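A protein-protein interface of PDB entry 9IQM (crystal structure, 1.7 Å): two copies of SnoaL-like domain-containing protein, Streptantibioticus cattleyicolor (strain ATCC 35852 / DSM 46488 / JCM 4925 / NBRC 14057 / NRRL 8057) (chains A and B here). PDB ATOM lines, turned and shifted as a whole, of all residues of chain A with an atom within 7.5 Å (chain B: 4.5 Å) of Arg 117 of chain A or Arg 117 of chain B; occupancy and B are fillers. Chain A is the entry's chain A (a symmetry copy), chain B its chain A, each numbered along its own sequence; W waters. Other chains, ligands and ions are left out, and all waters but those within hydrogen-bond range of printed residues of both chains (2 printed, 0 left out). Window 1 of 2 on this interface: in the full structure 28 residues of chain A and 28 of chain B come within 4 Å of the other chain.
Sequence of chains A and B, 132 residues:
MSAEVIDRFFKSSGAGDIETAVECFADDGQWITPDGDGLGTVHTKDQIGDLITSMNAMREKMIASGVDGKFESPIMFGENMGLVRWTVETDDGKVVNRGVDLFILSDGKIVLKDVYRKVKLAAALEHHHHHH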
ATOM      1  N   THR A  33      -7.726  31.517 -20.818  1.00  0.00           N
ATOM      2  CA  THR A  33      -6.721  30.460 -20.797  1.00  0.00           C
ATOM      3  C   THR A  33      -6.528  29.962 -19.375  1.00  0.00           C
ATOM      4  O   THR A  33      -6.952  30.604 -18.403  1.00  0.00           O
ATOM      5  CB  THR A  33      -5.374  30.947 -21.335  1.00  0.00           C
ATOM      6  OG1 THR A  33      -4.842  31.923 -20.435  1.00  0.00           O
ATOM      7  CG2 THR A  33      -5.525  31.553 -22.720  1.00  0.00           C
ATOM      8  N   PRO A  34      -5.865  28.818 -19.210  1.00  0.00           N
ATOM      9  CA  PRO A  34      -5.702  28.251 -17.875  1.00  0.00           C
ATOM     10  C   PRO A  34      -4.578  28.859 -17.067  1.00  0.00           C
ATOM     11  O   PRO A  34      -4.425  28.483 -15.903  1.00  0.00           O
ATOM     12  CB  PRO A  34      -5.424  26.765 -18.152  1.00  0.00           C
ATOM     13  CG  PRO A  34      -4.853  26.732 -19.547  1.00  0.00           C
ATOM     14  CD  PRO A  34      -5.537  27.856 -20.280  1.00  0.00           C
ATOM     15  N   ASP A  35      -3.759  29.747 -17.644  1.00  0.00           N
ATOM     16  CA  ASP A  35      -2.561  30.207 -16.955  1.00  0.00           C
ATOM     17  C   ASP A  35      -2.729  31.679 -16.623  1.00  0.00           C
ATOM     18  O   ASP A  35      -3.425  32.008 -15.635  1.00  0.00           O
ATOM     19  CB  ASP A  35      -1.324  29.913 -17.821  1.00  0.00           C
ATOM     20  CG  ASP A  35      -1.274  28.463 -18.273  1.00  0.00           C
ATOM     21  OD1 ASP A  35      -1.764  27.598 -17.511  1.00  0.00           O
ATOM     22  OD2 ASP A  35      -0.794  28.193 -19.396  1.00  0.00           O
ATOM     23  N   GLY A  38      -1.830  33.198 -12.880  1.00  0.00           N
ATOM     24  CA  GLY A  38      -2.705  32.801 -11.806  1.00  0.00           C
ATOM     25  C   GLY A  38      -4.114  33.347 -11.905  1.00  0.00           C
ATOM     26  O   GLY A  38      -4.923  33.079 -11.017  1.00  0.00           O
ATOM     27  N   LEU A  39      -4.422  34.129 -12.935  1.00  0.00           N
ATOM     28  CA  LEU A  39      -5.748  34.705 -13.076  1.00  0.00           C
ATOM     29  C   LEU A  39      -6.454  34.280 -14.348  1.00  0.00           C
ATOM     30  O   LEU A  39      -7.669  34.493 -14.459  1.00  0.00           O
ATOM     31  CB  LEU A  39      -5.663  36.239 -13.025  1.00  0.00           C
ATOM     32  CG  LEU A  39      -4.978  36.828 -11.796  1.00  0.00           C
ATOM     33  CD1 LEU A  39      -4.870  38.332 -11.902  1.00  0.00           C
ATOM     34  CD2 LEU A  39      -5.756  36.457 -10.546  1.00  0.00           C
ATOM     35  N   GLY A  40      -5.756  33.633 -15.274  1.00  0.00           N
ATOM     36  CA  GLY A  40      -6.304  33.338 -16.582  1.00  0.00           C
ATOM     37  C   GLY A  40      -6.144  34.549 -17.477  1.00  0.00           C
ATOM     38  O   GLY A  40      -6.198  35.689 -17.004  1.00  0.00           O
ATOM     39  N   TRP A  86     -10.023  16.860 -20.894  1.00  0.00           N
ATOM     40  CA  TRP A  86      -8.914  16.564 -21.792  1.00  0.00           C
ATOM     41  C   TRP A  86      -7.710  16.073 -21.013  1.00  0.00           C
ATOM     42  O   TRP A  86      -7.616  16.229 -19.793  1.00  0.00           O
ATOM     43  CB  TRP A  86      -8.494  17.769 -22.639  1.00  0.00           C
ATOM     44  CG  TRP A  86      -8.240  19.034 -21.914  1.00  0.00           C
ATOM     45  CD1 TRP A  86      -9.106  20.076 -21.774  1.00  0.00           C
ATOM     46  CD2 TRP A  86      -7.042  19.412 -21.227  1.00  0.00           C
ATOM     47  NE1 TRP A  86      -8.523  21.082 -21.044  1.00  0.00           N
ATOM     48  CE2 TRP A  86      -7.256  20.702 -20.693  1.00  0.00           C
ATOM     49  CE3 TRP A  86      -5.800  18.792 -21.025  1.00  0.00           C
ATOM     50  CZ2 TRP A  86      -6.276  21.383 -19.967  1.00  0.00           C
ATOM     51  CZ3 TRP A  86      -4.837  19.450 -20.288  1.00  0.00           C
ATOM     52  CH2 TRP A  86      -5.077  20.741 -19.765  1.00  0.00           C
ATOM     53  N   VAL A  88      -3.233  15.647 -21.605  1.00  0.00           N
ATOM     54  CA  VAL A  88      -2.001  15.621 -22.390  1.00  0.00           C
ATOM     55  C   VAL A  88      -1.335  14.285 -22.115  1.00  0.00           C
ATOM     56  O   VAL A  88      -1.119  13.924 -20.957  1.00  0.00           O
ATOM     57  CB  VAL A  88      -1.070  16.785 -22.024  1.00  0.00           C
ATOM     58  CG1 VAL A  88       0.188  16.725 -22.868  1.00  0.00           C
ATOM     59  CG2 VAL A  88      -1.737  18.118 -22.222  1.00  0.00           C
ATOM     60  N   ASN A  97      -0.814  15.464 -17.911  1.00  0.00           N
ATOM     61  CA  ASN A  97      -1.600  16.620 -17.491  1.00  0.00           C
ATOM     62  C   ASN A  97      -3.049  16.343 -17.856  1.00  0.00           C
ATOM     63  O   ASN A  97      -3.344  15.662 -18.841  1.00  0.00           O
ATOM     64  CB  ASN A  97      -1.086  17.897 -18.182  1.00  0.00           C
ATOM     65  CG  ASN A  97      -1.562  19.197 -17.537  1.00  0.00           C
ATOM     66  OD1 ASN A  97      -1.724  20.197 -18.237  1.00  0.00           O
ATOM     67  ND2 ASN A  97      -1.754  19.207 -16.215  1.00  0.00           N
ATOM     68  N   ARG A  98      -3.957  16.847 -17.034  1.00  0.00           N
ATOM     69  CA  ARG A  98      -5.353  16.776 -17.403  1.00  0.00           C
ATOM     70  C   ARG A  98      -6.027  18.068 -16.996  1.00  0.00           C
ATOM     71  O   ARG A  98      -5.511  18.839 -16.189  1.00  0.00           O
ATOM     72  CB  ARG A  98      -6.038  15.552 -16.786  1.00  0.00           C
ATOM     73  CG  ARG A  98      -5.988  15.447 -15.302  1.00  0.00           C
ATOM     74  CD  ARG A  98      -6.885  14.245 -14.857  1.00  0.00           C
ATOM     75  NE  ARG A  98      -6.179  12.966 -14.833  1.00  0.00           N
ATOM     76  CZ  ARG A  98      -6.289  12.017 -15.758  1.00  0.00           C
ATOM     77  NH1 ARG A  98      -7.012  12.190 -16.856  1.00  0.00           N
ATOM     78  NH2 ARG A  98      -5.676  10.855 -15.568  1.00  0.00           N
ATOM     79  N   GLY A  99      -7.163  18.327 -17.619  1.00  0.00           N
ATOM     80  CA  GLY A  99      -7.847  19.563 -17.321  1.00  0.00           C
ATOM     81  C   GLY A  99      -9.228  19.535 -17.919  1.00  0.00           C
ATOM     82  O   GLY A  99      -9.730  18.486 -18.324  1.00  0.00           O
ATOM     83  N   VAL A 100      -9.850  20.701 -17.961  1.00  0.00           N
ATOM     84  CA  VAL A 100     -11.221  20.792 -18.450  1.00  0.00           C
ATOM     85  C   VAL A 100     -11.382  22.077 -19.247  1.00  0.00           C
ATOM     86  O   VAL A 100     -10.702  23.076 -18.999  1.00  0.00           O
ATOM     87  CB  VAL A 100     -12.261  20.745 -17.311  1.00  0.00           C
ATOM     88  CG1 VAL A 100     -12.239  19.419 -16.598  1.00  0.00           C
ATOM     89  CG2 VAL A 100     -12.122  21.898 -16.367  1.00  0.00           C
ATOM     90  N   ASP A 101     -12.258  22.024 -20.250  1.00  0.00           N
ATOM     91  CA  ASP A 101     -12.808  23.189 -20.939  1.00  0.00           C
ATOM     92  C   ASP A 101     -14.267  23.320 -20.544  1.00  0.00           C
ATOM     93  O   ASP A 101     -15.038  22.397 -20.779  1.00  0.00           O
ATOM     94  CB  ASP A 101     -12.741  23.056 -22.465  1.00  0.00           C
ATOM     95  CG  ASP A 101     -11.348  23.009 -23.021  1.00  0.00           C
ATOM     96  OD1 ASP A 101     -10.369  23.106 -22.270  1.00  0.00           O
ATOM     97  OD2 ASP A 101     -11.251  22.817 -24.257  1.00  0.00           O
ATOM     98  N   VAL A 115     -10.869  27.590 -19.512  1.00  0.00           N
ATOM     99  CA  VAL A 115      -9.995  26.422 -19.530  1.00  0.00           C
ATOM    100  C   VAL A 115      -9.214  26.334 -18.233  1.00  0.00           C
ATOM    101  O   VAL A 115      -8.653  27.332 -17.776  1.00  0.00           O
ATOM    102  CB  VAL A 115      -9.027  26.496 -20.722  1.00  0.00           C
ATOM    103  CG1 VAL A 115      -8.217  25.217 -20.804  1.00  0.00           C
ATOM    104  CG2 VAL A 115      -9.817  26.721 -22.000  1.00  0.00           C
ATOM    105  N   TYR A 116      -9.131  25.121 -17.672  1.00  0.00           N
ATOM    106  CA  TYR A 116      -8.366  24.867 -16.458  1.00  0.00           C
ATOM    107  C   TYR A 116      -7.498  23.630 -16.625  1.00  0.00           C
ATOM    108  O   TYR A 116      -7.903  22.651 -17.249  1.00  0.00           O
ATOM    109  CB  TYR A 116      -9.291  24.655 -15.268  1.00  0.00           C
ATOM    110  CG  TYR A 116     -10.100  25.882 -14.974  1.00  0.00           C
ATOM    111  CD1 TYR A 116     -11.306  26.115 -15.612  1.00  0.00           C
ATOM    112  CD2 TYR A 116      -9.609  26.841 -14.112  1.00  0.00           C
ATOM    113  CE1 TYR A 116     -12.037  27.244 -15.352  1.00  0.00           C
ATOM    114  CE2 TYR A 116     -10.327  27.994 -13.847  1.00  0.00           C
ATOM    115  CZ  TYR A 116     -11.556  28.170 -14.467  1.00  0.00           C
ATOM    116  OH  TYR A 116     -12.270  29.324 -14.240  1.00  0.00           O
ATOM    117  N   ARG A 117      -6.338  23.651 -16.002  1.00  0.00           N
ATOM    118  CA  ARG A 117      -5.478  22.480 -15.975  1.00  0.00           C
ATOM    119  C   ARG A 117      -5.171  22.168 -14.523  1.00  0.00           C
ATOM    120  O   ARG A 117      -5.120  23.075 -13.691  1.00  0.00           O
ATOM    121  CB  ARG A 117      -4.167  22.731 -16.757  1.00  0.00           C
ATOM    122  CG  ARG A 117      -3.180  23.684 -16.037  1.00  0.00           C
ATOM    123  CD  ARG A 117      -1.755  23.705 -16.631  1.00  0.00           C
ATOM    124  NE  ARG A 117      -1.709  24.441 -17.890  1.00  0.00           N
ATOM    125  CZ  ARG A 117      -1.527  23.872 -19.075  1.00  0.00           C
ATOM    126  NH1 ARG A 117      -1.358  22.565 -19.193  1.00  0.00           N
ATOM    127  NH2 ARG A 117      -1.523  24.631 -20.167  1.00  0.00           N
ATOM    128  N   LYS A 118      -4.970  20.888 -14.215  1.00  0.00           N
ATOM    129  CA  LYS A 118      -4.376  20.559 -12.927  1.00  0.00           C
ATOM    130  C   LYS A 118      -2.929  21.045 -12.891  1.00  0.00           C
ATOM    131  O   LYS A 118      -2.226  21.061 -13.909  1.00  0.00           O
ATOM    132  CB  LYS A 118      -4.440  19.055 -12.664  1.00  0.00           C
ATOM    133  CG  LYS A 118      -5.871  18.474 -12.626  1.00  0.00           C
ATOM    134  CD  LYS A 118      -6.652  19.025 -11.435  1.00  0.00           C
ATOM    135  CE  LYS A 118      -8.045  18.378 -11.321  1.00  0.00           C
ATOM    136  NZ  LYS A 118      -8.806  18.930 -10.156  1.00  0.00           N
ATOM    137  N   VAL A 119      -2.501  21.447 -11.698  1.00  0.00           N
ATOM    138  CA  VAL A 119      -1.254  22.175 -11.471  1.00  0.00           C
ATOM    139  C   VAL A 119      -0.159  21.200 -11.069  1.00  0.00           C
ATOM    140  O   VAL A 119      -0.345  20.366 -10.174  1.00  0.00           O
ATOM    141  CB  VAL A 119      -1.437  23.244 -10.381  1.00  0.00           C
ATOM    142  CG1 VAL A 119      -0.099  23.864 -10.030  1.00  0.00           C
ATOM    143  CG2 VAL A 119      -2.422  24.315 -10.826  1.00  0.00           C
ATOM    144  N   LYS A 120       0.997  21.321 -11.710  1.00  0.00           N
ATOM    145  CA  LYS A 120       2.201  20.632 -11.280  1.00  0.00           C
ATOM    146  C   LYS A 120       2.996  21.614 -10.428  1.00  0.00           C
ATOM    147  O   LYS A 120       3.393  22.674 -10.919  1.00  0.00           O
ATOM    148  CB  LYS A 120       3.011  20.151 -12.484  1.00  0.00           C
ATOM    149  CG  LYS A 120       4.476  19.791 -12.210  1.00  0.00           C
ATOM    150  CD  LYS A 120       4.661  18.637 -11.223  1.00  0.00           C
ATOM    151  CE  LYS A 120       6.135  18.222 -11.141  1.00  0.00           C
ATOM    152  NZ  LYS A 120       6.421  17.159 -10.127  1.00  0.00           N
ATOM    153  N   LEU A 121       3.207  21.272  -9.162  1.00  0.00           N
ATOM    154  CA  LEU A 121       3.878  22.167  -8.228  1.00  0.00           C
ATOM    155  C   LEU A 121       5.356  21.816  -8.081  1.00  0.00           C
ATOM    156  O   LEU A 121       5.805  20.728  -8.454  1.00  0.00           O
ATOM    157  CB  LEU A 121       3.210  22.131  -6.847  1.00  0.00           C
ATOM    158  CG  LEU A 121       1.727  22.462  -6.681  1.00  0.00           C
ATOM    159  CD1 LEU A 121       1.284  22.172  -5.264  1.00  0.00           C
ATOM    160  CD2 LEU A 121       1.441  23.898  -7.046  1.00  0.00           C
ATOM    161  N   PRO B  34      -6.726  20.592  -6.966  1.00  0.00           N
ATOM    162  CA  PRO B  34      -6.310  21.240  -8.206  1.00  0.00           C
ATOM    163  C   PRO B  34      -4.871  20.989  -8.595  1.00  0.00           C
ATOM    164  O   PRO B  34      -4.467  21.442  -9.666  1.00  0.00           O
ATOM    165  CB  PRO B  34      -6.539  22.733  -7.921  1.00  0.00           C
ATOM    166  CG  PRO B  34      -6.465  22.855  -6.421  1.00  0.00           C
ATOM    167  CD  PRO B  34      -7.019  21.559  -5.891  1.00  0.00           C
ATOM    168  N   ASP B  35      -4.069  20.326  -7.751  1.00  0.00           N
ATOM    169  CA  ASP B  35      -2.639  20.233  -8.009  1.00  0.00           C
ATOM    170  C   ASP B  35      -2.296  18.784  -8.313  1.00  0.00           C
ATOM    171  O   ASP B  35      -2.533  18.325  -9.455  1.00  0.00           O
ATOM    172  CB  ASP B  35      -1.860  20.807  -6.813  1.00  0.00           C
ATOM    173  CG  ASP B  35      -2.342  22.196  -6.433  1.00  0.00           C
ATOM    174  OD1 ASP B  35      -2.780  22.932  -7.347  1.00  0.00           O
ATOM    175  OD2 ASP B  35      -2.328  22.535  -5.228  1.00  0.00           O
ATOM    176  N   TRP B  86     -14.226  30.928  -7.192  1.00  0.00           N
ATOM    177  CA  TRP B  86     -13.575  31.468  -6.006  1.00  0.00           C
ATOM    178  C   TRP B  86     -12.364  32.296  -6.389  1.00  0.00           C
ATOM    179  O   TRP B  86     -11.855  32.223  -7.511  1.00  0.00           O
ATOM    180  CB  TRP B  86     -13.137  30.383  -5.019  1.00  0.00           C
ATOM    181  CG  TRP B  86     -12.342  29.264  -5.572  1.00  0.00           C
ATOM    182  CD1 TRP B  86     -12.810  28.036  -5.930  1.00  0.00           C
ATOM    183  CD2 TRP B  86     -10.934  29.248  -5.832  1.00  0.00           C
ATOM    184  NE1 TRP B  86     -11.782  27.254  -6.397  1.00  0.00           N
ATOM    185  CE2 TRP B  86     -10.618  27.973  -6.350  1.00  0.00           C
ATOM    186  CE3 TRP B  86      -9.904  30.185  -5.661  1.00  0.00           C
ATOM    187  CZ2 TRP B  86      -9.317  27.610  -6.700  1.00  0.00           C
ATOM    188  CZ3 TRP B  86      -8.620  29.840  -6.029  1.00  0.00           C
ATOM    189  CH2 TRP B  86      -8.331  28.555  -6.544  1.00  0.00           C
ATOM    190  N   ASN B  97      -5.268  34.851  -7.199  1.00  0.00           N
ATOM    191  CA  ASN B  97      -5.546  33.548  -7.792  1.00  0.00           C
ATOM    192  C   ASN B  97      -7.054  33.413  -7.913  1.00  0.00           C
ATOM    193  O   ASN B  97      -7.813  33.947  -7.100  1.00  0.00           O
ATOM    194  CB  ASN B  97      -4.954  32.425  -6.920  1.00  0.00           C
ATOM    195  CG  ASN B  97      -4.840  31.074  -7.625  1.00  0.00           C
ATOM    196  OD1 ASN B  97      -4.940  30.039  -6.968  1.00  0.00           O
ATOM    197  ND2 ASN B  97      -4.597  31.071  -8.939  1.00  0.00           N
ATOM    198  N   ARG B  98      -7.491  32.723  -8.954  1.00  0.00           N
ATOM    199  CA  ARG B  98      -8.898  32.403  -9.045  1.00  0.00           C
ATOM    200  C   ARG B  98      -9.041  30.997  -9.586  1.00  0.00           C
ATOM    201  O   ARG B  98      -8.112  30.427 -10.156  1.00  0.00           O
ATOM    202  CB  ARG B  98      -9.654  33.426  -9.899  1.00  0.00           C
ATOM    203  CG  ARG B  98      -9.172  33.605 -11.294  1.00  0.00           C
ATOM    204  CD  ARG B  98     -10.170  34.544 -12.050  1.00  0.00           C
ATOM    205  NE  ARG B  98      -9.859  35.964 -11.907  1.00  0.00           N
ATOM    206  CZ  ARG B  98     -10.502  36.809 -11.105  1.00  0.00           C
ATOM    207  NH1 ARG B  98     -11.459  36.402 -10.283  1.00  0.00           N
ATOM    208  NH2 ARG B  98     -10.193  38.099 -11.144  1.00  0.00           N
ATOM    209  N   GLY B  99     -10.203  30.418  -9.340  1.00  0.00           N
ATOM    210  CA  GLY B  99     -10.404  29.059  -9.783  1.00  0.00           C
ATOM    211  C   GLY B  99     -11.858  28.692  -9.649  1.00  0.00           C
ATOM    212  O   GLY B  99     -12.721  29.552  -9.468  1.00  0.00           O
ATOM    213  N   TYR B 116     -10.206  23.350  -9.610  1.00  0.00           N
ATOM    214  CA  TYR B 116      -9.195  23.851 -10.532  1.00  0.00           C
ATOM    215  C   TYR B 116      -8.786  25.266 -10.156  1.00  0.00           C
ATOM    216  O   TYR B 116      -9.611  26.074  -9.734  1.00  0.00           O
ATOM    217  CB  TYR B 116      -9.723  23.861 -11.960  1.00  0.00           C
ATOM    218  CG  TYR B 116     -10.041  22.477 -12.440  1.00  0.00           C
ATOM    219  CD1 TYR B 116     -11.279  21.904 -12.202  1.00  0.00           C
ATOM    220  CD2 TYR B 116      -9.069  21.722 -13.061  1.00  0.00           C
ATOM    221  CE1 TYR B 116     -11.564  20.634 -12.627  1.00  0.00           C
ATOM    222  CE2 TYR B 116      -9.334  20.432 -13.488  1.00  0.00           C
ATOM    223  CZ  TYR B 116     -10.602  19.909 -13.276  1.00  0.00           C
ATOM    224  OH  TYR B 116     -10.874  18.618 -13.665  1.00  0.00           O
ATOM    225  N   ARG B 117      -7.528  25.582 -10.384  1.00  0.00           N
ATOM    226  CA  ARG B 117      -7.046  26.939 -10.190  1.00  0.00           C
ATOM    227  C   ARG B 117      -6.395  27.385 -11.485  1.00  0.00           C
ATOM    228  O   ARG B 117      -5.846  26.561 -12.219  1.00  0.00           O
ATOM    229  CB  ARG B 117      -6.030  27.012  -9.027  1.00  0.00           C
ATOM    230  CG  ARG B 117      -4.650  26.389  -9.360  1.00  0.00           C
ATOM    231  CD  ARG B 117      -3.533  26.722  -8.348  1.00  0.00           C
ATOM    232  NE  ARG B 117      -3.689  25.970  -7.107  1.00  0.00           N
ATOM    233  CZ  ARG B 117      -4.046  26.515  -5.952  1.00  0.00           C
ATOM    234  NH1 ARG B 117      -4.276  27.813  -5.844  1.00  0.00           N
ATOM    235  NH2 ARG B 117      -4.182  25.737  -4.880  1.00  0.00           N
ATOM    236  N   LYS B 118      -6.456  28.684 -11.770  1.00  0.00           N
ATOM    237  CA  LYS B 118      -5.598  29.215 -12.821  1.00  0.00           C
ATOM    238  C   LYS B 118      -4.139  29.134 -12.379  1.00  0.00           C
ATOM    239  O   LYS B 118      -3.813  29.261 -11.193  1.00  0.00           O
ATOM    240  CB  LYS B 118      -5.974  30.658 -13.156  1.00  0.00           C
ATOM    241  CG  LYS B 118      -7.422  30.838 -13.665  1.00  0.00           C
ATOM    242  CD  LYS B 118      -7.614  30.152 -15.016  1.00  0.00           C
ATOM    243  CE  LYS B 118      -9.020  30.410 -15.587  1.00  0.00           C
ATOM    244  NZ  LYS B 118      -9.203  29.726 -16.908  1.00  0.00           N
ATOM    245  N   VAL B 119      -3.268  28.913 -13.361  1.00  0.00           N
ATOM    246  CA  VAL B 119      -1.866  28.554 -13.154  1.00  0.00           C
ATOM    247  C   VAL B 119      -1.001  29.802 -13.233  1.00  0.00           C
ATOM    248  O   VAL B 119      -1.112  30.594 -14.178  1.00  0.00           O
ATOM    249  CB  VAL B 119      -1.407  27.523 -14.198  1.00  0.00           C
ATOM    250  CG1 VAL B 119       0.087  27.297 -14.085  1.00  0.00           C
ATOM    251  CG2 VAL B 119      -2.159  26.209 -14.038  1.00  0.00           C
HETATM  252  O   HOH W   1      -6.054  23.222 -11.184  1.00  0.00           O
HETATM  253  O   HOH W   2      -5.874  26.280 -14.883  1.00  0.00           O
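Water W2 lies within hydrogen-bond range of the backbone carbonyl oxygen of Arg 117 of chain B (2.7 Å), the backbone carbonyl oxygen of Pro 34 of chain A (2.8 Å) and the backbone NH of Arg 117 of chain A (2.9 Å). Water W1 lies within hydrogen-bond range of the backbone carbonyl oxygen of Arg 117 of chain A (2.7 Å), the backbone carbonyl oxygen of Pro 34 of chain B (2.8 Å) and the backbone NH of Arg 117 of chain B (2.9 Å).
N of Val 119 of chain A sits at hydrogen-bond distance from O of Pro 34 of chain B, 2.8 Å away. The side-chain amide nitrogen (ND2) of Asn 97 of chain B is in hydrogen-bond range of the backbone carbonyl oxygen (O) of Gly 38 of chain A (2.9 Å). The backbone NH (N) of Arg 98 of chain B is in hydrogen-bond range of the backbone carbonyl oxygen (O) of Gly 38 of chain A. The side-chain amino group (NZ) of Lys 118 of chain B lies within hydrogen-bond range of the backbone carbonyl oxygen (O) of Thr 33 of chain A, 2.8 Å away. NZ of Lys 118 of chain B lies within hydrogen-bond range of O of Val 115 of chain A (2.6 Å). The backbone carbonyl oxygen (O) of Pro 34 of chain A lies within hydrogen-bond range of the backbone NH (N) of Val 119 of chain B, 2.8 Å away. N of Gly 38 of chain A is in hydrogen-bond range of O of Val 119 of chain B. The backbone carbonyl oxygen (O) of Val 119 of chain B lies close to the backbone carbonyl oxygen (O) of Asp 35 of chain A (3.1 Å). O of Asp 35 of chain B lies close to O of Val 119 of chain A.
Pro 34 of chain A touches Val 119 of chain B, and with the chains exchanged Val 119 of chain A touches Pro 34 of chain B. Asp 35 of chain A touches Lys 118 of chain B, and with the chains exchanged Lys 118 of chain A touches Asp 35 of chain B. Asp 35 of chain A touches Val 119 of chain B, and with the chains exchanged Val 119 of chain A touches Asp 35 of chain B. Val 119 of chain B touches its own counterpart, Val 119 of chain A. Of the 27 pairs that touch across the chains among the printed residues, 15 have their exchanged pair printed and touching as well.
NH1 of Arg 117 of chain B sits at hydrogen-bond distance from OD1 of Asn 97 of chain B (2.6 Å). The backbone carbonyl oxygen (O) of Asp 35 of chain A sits at hydrogen-bond distance from the backbone NH (N) of Gly 40 of chain A (2.9 Å). The side-chain carboxylate (OD1) of Asp 35 of chain A is in salt-bridge range of the guanidinium group (NE) of Arg 117 of chain A, 3.2 Å away. The side-chain amide oxygen (OD1) of Asn 97 of chain A is in hydrogen-bond range of the guanidinium group (NH1) of Arg 117 of chain A, 2.6 Å away. The backbone NH of Lys 118 of chain A is in hydrogen-bond range of the backbone carbonyl oxygen of Arg 98 of chain A, 2.9 Å away. The backbone NH of Val 100 of chain A lies within hydrogen-bond range of the backbone carbonyl oxygen of Tyr 116 of chain A (2.8 Å).
Of the 10 printed residues of chain B, 8 touch a printed residue of chain A. Along chain B the printed residues that touch a printed residue of chain A span positions 34 to 119.
Gly 99 of chain A touches none of the printed residues of chain B. Of chain B, only Arg 117 (3.9 Å) and Val 119 (3.4 Å) come within 4 Å of Arg 117 of chain A. Printed residues of chain B within 4 Å of Lys 118 of chain A: Pro 34, Asp 35 and Tyr 116. Of the printed residues of chain A, Asn 97 of chain B touches Gly 38 and Leu 39.
Among the printed residues, merely in contact across the chains: Tyr 116 of chain A with Lys 118 of chain B, Lys 118 of chain A with Tyr 116 of chain B, Val 100 of chain A with Tyr 116 of chain B, Pro 34 of chain A with Lys 118 of chain B, Arg 117 of chain A with Val 119 of chain B, Val 119 of chain A with Arg 117 of chain B, Lys 118 of chain A with Pro 34 of chain B, Gly 38 of chain A with Lys 118 of chain B, Tyr 116 of chain A with Tyr 116 of chain B, Leu 39 of chain A with Arg 98 of chain B, Gly 40 of chain A with Lys 118 of chain B, Leu 121 of chain A with Asp 35 of chain B, Leu 39 of chain A with Lys 118 of chain B, Val 119 of chain A with Val 119 of chain B, Leu 39 of chain A with Asn 97 of chain B, Asp 35 of chain A with Lys 118 of chain B, Lys 118 of chain A with Asp 35 of chain B and Arg 117 of chain A with Arg 117 of chain B.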
